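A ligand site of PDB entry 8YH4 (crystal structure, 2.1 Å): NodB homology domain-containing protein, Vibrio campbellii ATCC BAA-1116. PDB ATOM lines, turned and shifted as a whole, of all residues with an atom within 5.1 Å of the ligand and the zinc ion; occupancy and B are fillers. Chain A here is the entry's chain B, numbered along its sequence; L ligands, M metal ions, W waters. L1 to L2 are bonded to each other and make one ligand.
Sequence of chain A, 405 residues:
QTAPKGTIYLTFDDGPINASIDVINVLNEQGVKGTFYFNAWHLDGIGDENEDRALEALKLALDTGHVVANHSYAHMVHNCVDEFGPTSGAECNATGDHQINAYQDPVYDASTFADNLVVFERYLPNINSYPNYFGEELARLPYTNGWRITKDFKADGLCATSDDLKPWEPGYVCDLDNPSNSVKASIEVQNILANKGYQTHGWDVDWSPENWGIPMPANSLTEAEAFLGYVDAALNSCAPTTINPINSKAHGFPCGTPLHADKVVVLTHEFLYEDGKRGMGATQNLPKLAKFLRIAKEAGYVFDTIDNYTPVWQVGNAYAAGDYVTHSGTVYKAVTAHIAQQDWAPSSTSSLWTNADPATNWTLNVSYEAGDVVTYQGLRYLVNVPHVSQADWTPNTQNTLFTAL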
ATOM      1  N   ASP A  13      37.907 -13.979 -12.021  1.00  0.00           N
ATOM      2  CA  ASP A  13      36.740 -14.007 -11.160  1.00  0.00           C
ATOM      3  C   ASP A  13      35.811 -15.153 -11.523  1.00  0.00           C
ATOM      4  O   ASP A  13      35.784 -15.620 -12.669  1.00  0.00           O
ATOM      5  CB  ASP A  13      35.967 -12.679 -11.261  1.00  0.00           C
ATOM      6  CG  ASP A  13      36.649 -11.543 -10.523  1.00  0.00           C
ATOM      7  OD1 ASP A  13      37.828 -11.713 -10.134  1.00  0.00           O
ATOM      8  OD2 ASP A  13      36.007 -10.484 -10.342  1.00  0.00           O
ATOM      9  N   ASP A  14      35.069 -15.621 -10.509  1.00  0.00           N
ATOM     10  CA  ASP A  14      33.882 -16.466 -10.621  1.00  0.00           C
ATOM     11  C   ASP A  14      34.185 -17.958 -10.750  1.00  0.00           C
ATOM     12  O   ASP A  14      33.266 -18.758 -10.962  1.00  0.00           O
ATOM     13  CB  ASP A  14      33.011 -16.016 -11.797  1.00  0.00           C
ATOM     14  CG  ASP A  14      32.448 -14.626 -11.591  1.00  0.00           C
ATOM     15  OD1 ASP A  14      32.977 -13.885 -10.729  1.00  0.00           O
ATOM     16  OD2 ASP A  14      31.463 -14.272 -12.271  1.00  0.00           O
ATOM     17  N   ASN A  39      34.209 -18.248  -5.959  1.00  0.00           N
ATOM     18  CA  ASN A  39      32.903 -18.432  -5.333  1.00  0.00           C
ATOM     19  C   ASN A  39      32.741 -19.919  -5.048  1.00  0.00           C
ATOM     20  O   ASN A  39      32.684 -20.726  -5.984  1.00  0.00           O
ATOM     21  CB  ASN A  39      31.766 -17.946  -6.234  1.00  0.00           C
ATOM     22  CG  ASN A  39      31.980 -16.525  -6.718  1.00  0.00           C
ATOM     23  OD1 ASN A  39      32.142 -16.286  -7.916  1.00  0.00           O
ATOM     24  ND2 ASN A  39      31.941 -15.566  -5.804  1.00  0.00           N
ATOM     25  N   TRP A  41      30.312 -21.761  -4.219  1.00  0.00           N
ATOM     26  CA  TRP A  41      29.103 -22.492  -4.578  1.00  0.00           C
ATOM     27  C   TRP A  41      29.332 -23.418  -5.772  1.00  0.00           C
ATOM     28  O   TRP A  41      28.594 -24.383  -5.954  1.00  0.00           O
ATOM     29  CB  TRP A  41      27.920 -21.542  -4.854  1.00  0.00           C
ATOM     30  CG  TRP A  41      28.027 -20.676  -6.085  1.00  0.00           C
ATOM     31  CD1 TRP A  41      29.159 -20.196  -6.664  1.00  0.00           C
ATOM     32  CD2 TRP A  41      26.931 -20.169  -6.859  1.00  0.00           C
ATOM     33  NE1 TRP A  41      28.841 -19.426  -7.764  1.00  0.00           N
ATOM     34  CE2 TRP A  41      27.473 -19.389  -7.907  1.00  0.00           C
ATOM     35  CE3 TRP A  41      25.535 -20.308  -6.784  1.00  0.00           C
ATOM     36  CZ2 TRP A  41      26.682 -18.751  -8.863  1.00  0.00           C
ATOM     37  CZ3 TRP A  41      24.752 -19.664  -7.739  1.00  0.00           C
ATOM     38  CH2 TRP A  41      25.325 -18.897  -8.754  1.00  0.00           C
ATOM     39  N   HIS A  42      30.379 -23.155  -6.563  1.00  0.00           N
ATOM     40  CA  HIS A  42      30.746 -24.089  -7.622  1.00  0.00           C
ATOM     41  C   HIS A  42      31.260 -25.397  -7.054  1.00  0.00           C
ATOM     42  O   HIS A  42      31.090 -26.453  -7.673  1.00  0.00           O
ATOM     43  CB  HIS A  42      31.797 -23.453  -8.523  1.00  0.00           C
ATOM     44  CG  HIS A  42      31.311 -22.252  -9.265  1.00  0.00           C
ATOM     45  ND1 HIS A  42      30.287 -22.305 -10.193  1.00  0.00           N
ATOM     46  CD2 HIS A  42      31.715 -20.954  -9.232  1.00  0.00           C
ATOM     47  CE1 HIS A  42      30.086 -21.100 -10.683  1.00  0.00           C
ATOM     48  NE2 HIS A  42      30.925 -20.263 -10.115  1.00  0.00           N
ATOM     49  N   GLY A  47      26.335 -23.766  -9.062  1.00  0.00           N
ATOM     50  CA  GLY A  47      26.682 -22.525  -9.723  1.00  0.00           C
ATOM     51  C   GLY A  47      26.323 -22.425 -11.186  1.00  0.00           C
ATOM     52  O   GLY A  47      26.658 -21.428 -11.821  1.00  0.00           O
ATOM     53  N   GLU A  49      27.516 -23.846 -13.835  1.00  0.00           N
ATOM     54  CA  GLU A  49      28.604 -23.928 -14.791  1.00  0.00           C
ATOM     55  C   GLU A  49      29.052 -25.387 -14.882  1.00  0.00           C
ATOM     56  O   GLU A  49      28.660 -26.224 -14.073  1.00  0.00           O
ATOM     57  CB  GLU A  49      29.786 -23.031 -14.395  1.00  0.00           C
ATOM     58  CG  GLU A  49      29.427 -21.566 -14.172  1.00  0.00           C
ATOM     59  CD  GLU A  49      29.037 -20.865 -15.455  1.00  0.00           C
ATOM     60  OE1 GLU A  49      29.343 -21.386 -16.548  1.00  0.00           O
ATOM     61  OE2 GLU A  49      28.424 -19.775 -15.370  1.00  0.00           O
ATOM     62  N   HIS A  71      35.531 -14.081  -3.125  1.00  0.00           N
ATOM     63  CA  HIS A  71      34.580 -13.396  -3.995  1.00  0.00           C
ATOM     64  C   HIS A  71      33.131 -13.589  -3.536  1.00  0.00           C
ATOM     65  O   HIS A  71      32.215 -13.261  -4.300  1.00  0.00           O
ATOM     66  CB  HIS A  71      34.758 -13.895  -5.433  1.00  0.00           C
ATOM     67  CG  HIS A  71      34.248 -12.942  -6.473  1.00  0.00           C
ATOM     68  ND1 HIS A  71      34.282 -11.575  -6.315  1.00  0.00           N
ATOM     69  CD2 HIS A  71      33.715 -13.162  -7.700  1.00  0.00           C
ATOM     70  CE1 HIS A  71      33.788 -10.995  -7.384  1.00  0.00           C
ATOM     71  NE2 HIS A  71      33.438 -11.928  -8.247  1.00  0.00           N
ATOM     72  N   HIS A  75      28.128 -15.289  -5.128  1.00  0.00           N
ATOM     73  CA  HIS A  75      28.155 -14.126  -6.019  1.00  0.00           C
ATOM     74  C   HIS A  75      26.916 -13.256  -5.852  1.00  0.00           C
ATOM     75  O   HIS A  75      26.465 -12.605  -6.801  1.00  0.00           O
ATOM     76  CB  HIS A  75      28.307 -14.570  -7.477  1.00  0.00           C
ATOM     77  CG  HIS A  75      29.009 -13.582  -8.355  1.00  0.00           C
ATOM     78  ND1 HIS A  75      28.372 -12.513  -8.939  1.00  0.00           N
ATOM     79  CD2 HIS A  75      30.298 -13.504  -8.758  1.00  0.00           C
ATOM     80  CE1 HIS A  75      29.234 -11.825  -9.656  1.00  0.00           C
ATOM     81  NE2 HIS A  75      30.415 -12.397  -9.561  1.00  0.00           N
ATOM     82  N   VAL A  77      23.918 -14.127  -5.574  1.00  0.00           N
ATOM     83  CA  VAL A  77      22.784 -14.603  -6.365  1.00  0.00           C
ATOM     84  C   VAL A  77      21.564 -14.867  -5.492  1.00  0.00           C
ATOM     85  O   VAL A  77      20.442 -14.906  -5.997  1.00  0.00           O
ATOM     86  CB  VAL A  77      23.232 -15.831  -7.190  1.00  0.00           C
ATOM     87  CG1 VAL A  77      22.046 -16.539  -7.828  1.00  0.00           C
ATOM     88  CG2 VAL A  77      24.211 -15.401  -8.270  1.00  0.00           C
ATOM     89  N   ASN A  93      20.486 -16.867 -14.296  1.00  0.00           N
ATOM     90  CA  ASN A  93      21.031 -16.847 -15.647  1.00  0.00           C
ATOM     91  C   ASN A  93      19.927 -16.750 -16.696  1.00  0.00           C
ATOM     92  O   ASN A  93      20.132 -16.154 -17.760  1.00  0.00           O
ATOM     93  CB  ASN A  93      21.890 -18.084 -15.905  1.00  0.00           C
ATOM     94  CG  ASN A  93      23.312 -17.925 -15.412  1.00  0.00           C
ATOM     95  OD1 ASN A  93      23.824 -16.805 -15.307  1.00  0.00           O
ATOM     96  ND2 ASN A  93      23.969 -19.035 -15.100  1.00  0.00           N
ATOM     97  N   HIS A  98      21.340 -10.357 -12.674  1.00  0.00           N
ATOM     98  CA  HIS A  98      22.364 -10.427 -11.642  1.00  0.00           C
ATOM     99  C   HIS A  98      22.623  -9.070 -10.997  1.00  0.00           C
ATOM    100  O   HIS A  98      22.798  -8.975  -9.775  1.00  0.00           O
ATOM    101  CB  HIS A  98      23.671 -10.984 -12.228  1.00  0.00           C
ATOM    102  CG  HIS A  98      23.552 -12.361 -12.789  1.00  0.00           C
ATOM    103  ND1 HIS A  98      23.061 -12.613 -14.053  1.00  0.00           N
ATOM    104  CD2 HIS A  98      23.870 -13.578 -12.267  1.00  0.00           C
ATOM    105  CE1 HIS A  98      23.073 -13.911 -14.283  1.00  0.00           C
ATOM    106  NE2 HIS A  98      23.563 -14.518 -13.217  1.00  0.00           N
ATOM    107  N   GLN A  99      22.633  -8.004 -11.804  1.00  0.00           N
ATOM    108  CA  GLN A  99      22.959  -6.676 -11.305  1.00  0.00           C
ATOM    109  C   GLN A  99      21.810  -5.987 -10.584  1.00  0.00           C
ATOM    110  O   GLN A  99      22.029  -4.922 -10.000  1.00  0.00           O
ATOM    111  CB  GLN A  99      23.428  -5.791 -12.466  1.00  0.00           C
ATOM    112  CG  GLN A  99      24.934  -5.610 -12.567  1.00  0.00           C
ATOM    113  CD  GLN A  99      25.598  -6.644 -13.449  1.00  0.00           C
ATOM    114  OE1 GLN A  99      25.023  -7.691 -13.748  1.00  0.00           O
ATOM    115  NE2 GLN A  99      26.817  -6.346 -13.887  1.00  0.00           N
ATOM    116  N   PRO A 142      31.330  -8.803  -5.855  1.00  0.00           N
ATOM    117  CA  PRO A 142      30.695  -9.075  -7.146  1.00  0.00           C
ATOM    118  C   PRO A 142      30.137  -7.800  -7.771  1.00  0.00           C
ATOM    119  O   PRO A 142      29.519  -6.973  -7.097  1.00  0.00           O
ATOM    120  CB  PRO A 142      29.577 -10.058  -6.785  1.00  0.00           C
ATOM    121  CG  PRO A 142      30.126 -10.805  -5.598  1.00  0.00           C
ATOM    122  CD  PRO A 142      30.965  -9.802  -4.830  1.00  0.00           C
ATOM    123  N   TYR A 143      30.390  -7.647  -9.075  1.00  0.00           N
ATOM    124  CA  TYR A 143      29.856  -6.608  -9.952  1.00  0.00           C
ATOM    125  C   TYR A 143      30.456  -5.223  -9.732  1.00  0.00           C
ATOM    126  O   TYR A 143      30.136  -4.298 -10.482  1.00  0.00           O
ATOM    127  CB  TYR A 143      28.329  -6.458  -9.834  1.00  0.00           C
ATOM    128  CG  TYR A 143      27.584  -7.769  -9.773  1.00  0.00           C
ATOM    129  CD1 TYR A 143      27.544  -8.618 -10.871  1.00  0.00           C
ATOM    130  CD2 TYR A 143      26.918  -8.166  -8.607  1.00  0.00           C
ATOM    131  CE1 TYR A 143      26.858  -9.823 -10.808  1.00  0.00           C
ATOM    132  CE2 TYR A 143      26.235  -9.358  -8.543  1.00  0.00           C
ATOM    133  CZ  TYR A 143      26.214 -10.180  -9.657  1.00  0.00           C
ATOM    134  OH  TYR A 143      25.538 -11.379  -9.603  1.00  0.00           O
ATOM    135  N   TRP A 168      23.023  -1.579 -19.310  1.00  0.00           N
ATOM    136  CA  TRP A 168      23.037  -1.615 -20.761  1.00  0.00           C
ATOM    137  C   TRP A 168      21.658  -1.486 -21.374  1.00  0.00           C
ATOM    138  O   TRP A 168      21.531  -1.509 -22.608  1.00  0.00           O
ATOM    139  CB  TRP A 168      23.709  -2.908 -21.253  1.00  0.00           C
ATOM    140  CG  TRP A 168      23.215  -4.157 -20.578  1.00  0.00           C
ATOM    141  CD1 TRP A 168      22.138  -4.915 -20.935  1.00  0.00           C
ATOM    142  CD2 TRP A 168      23.780  -4.782 -19.423  1.00  0.00           C
ATOM    143  NE1 TRP A 168      21.994  -5.978 -20.081  1.00  0.00           N
ATOM    144  CE2 TRP A 168      22.989  -5.923 -19.137  1.00  0.00           C
ATOM    145  CE3 TRP A 168      24.865  -4.502 -18.598  1.00  0.00           C
ATOM    146  CZ2 TRP A 168      23.261  -6.777 -18.076  1.00  0.00           C
ATOM    147  CZ3 TRP A 168      25.139  -5.342 -17.536  1.00  0.00           C
ATOM    148  CH2 TRP A 168      24.332  -6.471 -17.281  1.00  0.00           C
ATOM    149  N   TRP A 212      27.738  -6.598 -20.540  1.00  0.00           N
ATOM    150  CA  TRP A 212      27.267  -7.939 -20.240  1.00  0.00           C
ATOM    151  C   TRP A 212      25.865  -8.221 -20.767  1.00  0.00           C
ATOM    152  O   TRP A 212      25.258  -9.225 -20.373  1.00  0.00           O
ATOM    153  CB  TRP A 212      27.327  -8.169 -18.725  1.00  0.00           C
ATOM    154  CG  TRP A 212      28.738  -8.341 -18.282  1.00  0.00           C
ATOM    155  CD1 TRP A 212      29.540  -7.407 -17.693  1.00  0.00           C
ATOM    156  CD2 TRP A 212      29.542  -9.505 -18.451  1.00  0.00           C
ATOM    157  NE1 TRP A 212      30.787  -7.927 -17.457  1.00  0.00           N
ATOM    158  CE2 TRP A 212      30.814  -9.219 -17.907  1.00  0.00           C
ATOM    159  CE3 TRP A 212      29.307 -10.779 -18.988  1.00  0.00           C
ATOM    160  CZ2 TRP A 212      31.843 -10.163 -17.899  1.00  0.00           C
ATOM    161  CZ3 TRP A 212      30.325 -11.707 -18.980  1.00  0.00           C
ATOM    162  CH2 TRP A 212      31.578 -11.398 -18.427  1.00  0.00           C
ATOM    163  N   LEU A 267      41.134  -7.591 -14.987  1.00  0.00           N
ATOM    164  CA  LEU A 267      40.038  -8.482 -14.638  1.00  0.00           C
ATOM    165  C   LEU A 267      39.622  -9.287 -15.864  1.00  0.00           C
ATOM    166  O   LEU A 267      39.521  -8.742 -16.973  1.00  0.00           O
ATOM    167  CB  LEU A 267      38.837  -7.700 -14.109  1.00  0.00           C
ATOM    168  CG  LEU A 267      37.476  -8.387 -14.171  1.00  0.00           C
ATOM    169  CD1 LEU A 267      37.410  -9.576 -13.215  1.00  0.00           C
ATOM    170  CD2 LEU A 267      36.334  -7.418 -13.877  1.00  0.00           C
ATOM    171  N   HIS A 269      37.347 -13.396 -16.662  1.00  0.00           N
ATOM    172  CA  HIS A 269      36.590 -14.505 -16.087  1.00  0.00           C
ATOM    173  C   HIS A 269      36.951 -15.783 -16.833  1.00  0.00           C
ATOM    174  O   HIS A 269      36.926 -15.793 -18.065  1.00  0.00           O
ATOM    175  CB  HIS A 269      35.083 -14.258 -16.164  1.00  0.00           C
ATOM    176  CG  HIS A 269      34.645 -12.966 -15.557  1.00  0.00           C
ATOM    177  ND1 HIS A 269      34.813 -11.756 -16.198  1.00  0.00           N
ATOM    178  CD2 HIS A 269      34.035 -12.691 -14.388  1.00  0.00           C
ATOM    179  CE1 HIS A 269      34.329 -10.791 -15.432  1.00  0.00           C
ATOM    180  NE2 HIS A 269      33.841 -11.332 -14.335  1.00  0.00           N
ATOM    181  N   PHE A 271      35.218 -18.334 -17.207  1.00  0.00           N
ATOM    182  CA  PHE A 271      34.124 -18.880 -17.998  1.00  0.00           C
ATOM    183  C   PHE A 271      34.093 -18.317 -19.420  1.00  0.00           C
ATOM    184  O   PHE A 271      33.300 -18.792 -20.236  1.00  0.00           O
ATOM    185  CB  PHE A 271      32.750 -18.679 -17.307  1.00  0.00           C
ATOM    186  CG  PHE A 271      32.327 -17.224 -17.102  1.00  0.00           C
ATOM    187  CD1 PHE A 271      32.077 -16.379 -18.181  1.00  0.00           C
ATOM    188  CD2 PHE A 271      32.089 -16.748 -15.823  1.00  0.00           C
ATOM    189  CE1 PHE A 271      31.651 -15.075 -17.974  1.00  0.00           C
ATOM    190  CE2 PHE A 271      31.656 -15.449 -15.617  1.00  0.00           C
ATOM    191  CZ  PHE A 271      31.447 -14.611 -16.692  1.00  0.00           C
ATOM    192  N   ARG A 278      28.495 -19.756 -24.053  1.00  0.00           N
ATOM    193  CA  ARG A 278      28.870 -18.371 -24.260  1.00  0.00           C
ATOM    194  C   ARG A 278      29.696 -18.156 -25.520  1.00  0.00           C
ATOM    195  O   ARG A 278      30.085 -17.012 -25.810  1.00  0.00           O
ATOM    196  CB  ARG A 278      29.661 -17.852 -23.050  1.00  0.00           C
ATOM    197  CG  ARG A 278      28.843 -17.775 -21.774  1.00  0.00           C
ATOM    198  CD  ARG A 278      29.709 -17.313 -20.619  1.00  0.00           C
ATOM    199  NE  ARG A 278      28.961 -17.223 -19.374  1.00  0.00           N
ATOM    200  CZ  ARG A 278      28.854 -18.209 -18.482  1.00  0.00           C
ATOM    201  NH1 ARG A 278      29.464 -19.367 -18.712  1.00  0.00           N
ATOM    202  NH2 ARG A 278      28.155 -18.037 -17.379  1.00  0.00           N
HETATM  203  C1  LIG L   1      30.167  -8.287 -14.068  1.00  0.00           C
HETATM  204  C2  LIG L   1      30.674  -9.356 -13.105  1.00  0.00           C
HETATM  205  C3  LIG L   1      30.523 -10.744 -13.730  1.00  0.00           C
HETATM  206  C4  LIG L   1      29.097 -10.968 -14.217  1.00  0.00           C
HETATM  207  C5  LIG L   1      28.662  -9.821 -15.118  1.00  0.00           C
HETATM  208  C6  LIG L   1      27.218  -9.896 -15.547  1.00  0.00           C
HETATM  209  N1  LIG L   1      32.059  -9.103 -12.743  1.00  0.00           N
HETATM  210  O1  LIG L   1      30.245  -7.051 -13.459  1.00  0.00           O
HETATM  211  O2  LIG L   1      30.877 -11.726 -12.759  1.00  0.00           O
HETATM  212  O3  LIG L   1      29.040 -12.192 -14.944  1.00  0.00           O
HETATM  213  O4  LIG L   1      28.820  -8.574 -14.429  1.00  0.00           O
HETATM  214  O5  LIG L   1      26.338 -10.041 -14.441  1.00  0.00           O
HETATM  215  C1  LG2 L   2      28.041 -13.069 -14.383  1.00  0.00           C
HETATM  216  C2  LG2 L   2      27.689 -14.108 -15.474  1.00  0.00           C
HETATM  217  C3  LG2 L   2      26.666 -15.103 -14.932  1.00  0.00           C
HETATM  218  C4  LG2 L   2      27.181 -15.737 -13.642  1.00  0.00           C
HETATM  219  C5  LG2 L   2      27.548 -14.652 -12.638  1.00  0.00           C
HETATM  220  C6  LG2 L   2      28.172 -15.207 -11.383  1.00  0.00           C
HETATM  221  N1  LG2 L   2      27.178 -13.445 -16.671  1.00  0.00           N
HETATM  222  O1  LG2 L   2      26.432 -16.103 -15.907  1.00  0.00           O
HETATM  223  O2  LG2 L   2      26.181 -16.578 -13.089  1.00  0.00           O
HETATM  224  O3  LG2 L   2      28.509 -13.753 -13.212  1.00  0.00           O
HETATM  225  O4  LG2 L   2      29.339 -15.971 -11.683  1.00  0.00           O
HETATM  226 ZN    ZN M   1      32.318 -11.901 -10.208  1.00  0.00          ZN
HETATM  227  O   HOH W   1      29.631 -18.547 -12.788  1.00  0.00           O
HETATM  228  O   HOH W   2      26.634 -19.220 -13.597  1.00  0.00           O
HETATM  229  O   HOH W   3      33.473 -10.725 -11.361  1.00  0.00           O
HETATM  230  O   HOH W   4      23.558 -17.095 -12.037  1.00  0.00           O
HETATM  231  O   HOH W   5      27.554 -15.060 -19.075  1.00  0.00           O
HETATM  232  O   HOH W   6      31.234  -5.013 -14.905  1.00  0.00           O
HETATM  233  O   HOH W   7      32.911  -7.328 -15.859  1.00  0.00           O
HETATM  234  O   HOH W   8      31.778  -9.804 -10.122  1.00  0.00           O
HETATM  235  O   HOH W   9      24.057 -10.779 -15.983  1.00  0.00           O
HETATM  236  O   HOH W  10      30.359 -17.494  -9.642  1.00  0.00           O
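Water W2 lies within hydrogen-bond range of the side-chain carboxylate (OE2) of Glu 49 (2.6 Å), an oxygen (O2) of LG2 L2 (2.7 Å), the backbone carbonyl oxygen (O) of Gly 47 (2.8 Å) and the side-chain amide nitrogen (ND2) of Asn 93 (3.1 Å).
Water W10 lies within hydrogen-bond range of an oxygen (O4) of LG2 L2 (2.7 Å), the side-chain amide oxygen (OD1) of Asn 39 (2.8 Å), a ring nitrogen (NE2) of His 42 (2.9 Å), the indole nitrogen (NE1) of Trp 41 (3.1 Å) and the backbone carbonyl oxygen (O) of Asp 14 (3.4 Å).
Water W1 lies within hydrogen-bond range of O4 of LG2 L2 (2.8 Å), OE2 of Glu 49 (3.1 Å) and NE2 of His 42 (3.4 Å).
Water W9 lies within hydrogen-bond range of a ring nitrogen (ND1) of His 98 and an oxygen (O5) of LIG L1.
Water W4 lies within hydrogen-bond range of NE2 of His 98 (2.8 Å), O2 of LG2 L2 (2.9 Å) and OD1 of Asn 93 (3.3 Å).
Water W5 bridges NE of Arg 278 (2.6 Å) and N1 of LG2 L2 (2.9 Å).
Merely in contact with the ligand: Tyr 143 (3.6 Å), Trp 212 (3.5 Å) and Phe 271 (3.8 Å).
Hydrophobic or aromatic side chains that line the ligand: His 75, His 98, Tyr 143, Trp 212, His 269 and Phe 271.
Within 4 Å of the ligand: Asp 14, His 75, Asn 93, His 98, Gln 99, Tyr 143, Trp 212, His 269, Phe 271 and Arg 278.
The nearest printed residue that does not touch the ligand is Glu 49 (4.2 Å).
CB of Asp 13 touches the zinc ion, at 3.9 Å.
Of the 21 residues printed, 4 come within 4 Å of the zinc ion.
The side-chain amide oxygen of Asn 93 is in hydrogen-bond range of an oxygen (O1) of LG2 L2 (2.8 Å).
O1 of LG2 L2 is in hydrogen-bond range of NH2 of Arg 278, 3.0 Å away.
NE2 of His 98 sits at hydrogen-bond distance from O2 of LG2 L2 (3.3 Å).
A ring nitrogen (NE2) of His 269 is in hydrogen-bond range of a nitrogen (N1) of LIG L1 (3.3 Å).
An oxygen (O5) of LIG L1 lies within hydrogen-bond range of the side-chain amide oxygen (OE1) of Gln 99 (2.8 Å).
An oxygen (O2) of LIG L1 lies close to a ring nitrogen (NE2) of His 75, at 3.3 Å.
The side-chain carboxylate of Asp 14 sits at hydrogen-bond distance from an oxygen (O2) of LIG L1, 2.7 Å away.
A ring nitrogen (NE2) of His 42 is in hydrogen-bond range of the backbone carbonyl oxygen (O) of Asp 14, 2.9 Å away.
NH2 of Arg 278 is in salt-bridge range of OE2 of Glu 49, 2.7 Å away.
OD1 of Asn 93 is in hydrogen-bond range of NE2 of His 98 (3.1 Å).
The side-chain hydroxyl (OH) of Tyr 143 sits at hydrogen-bond distance from a ring nitrogen (ND1) of His 75, at 3.1 Å.
O of His 71 sits at hydrogen-bond distance from ND2 of Asn 39 (2.8 Å).
Water W3 is bound to the zinc ion, at 2.0 Å.
NE2 of His 75 is bound to the zinc ion (2.1 Å).
The side-chain carboxylate (OD1) of Asp 14 binds the zinc ion (2.2 Å).
The zinc ion is bound by water W8.
The zinc ion is bound by NE2 of His 71 (2.3 Å).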
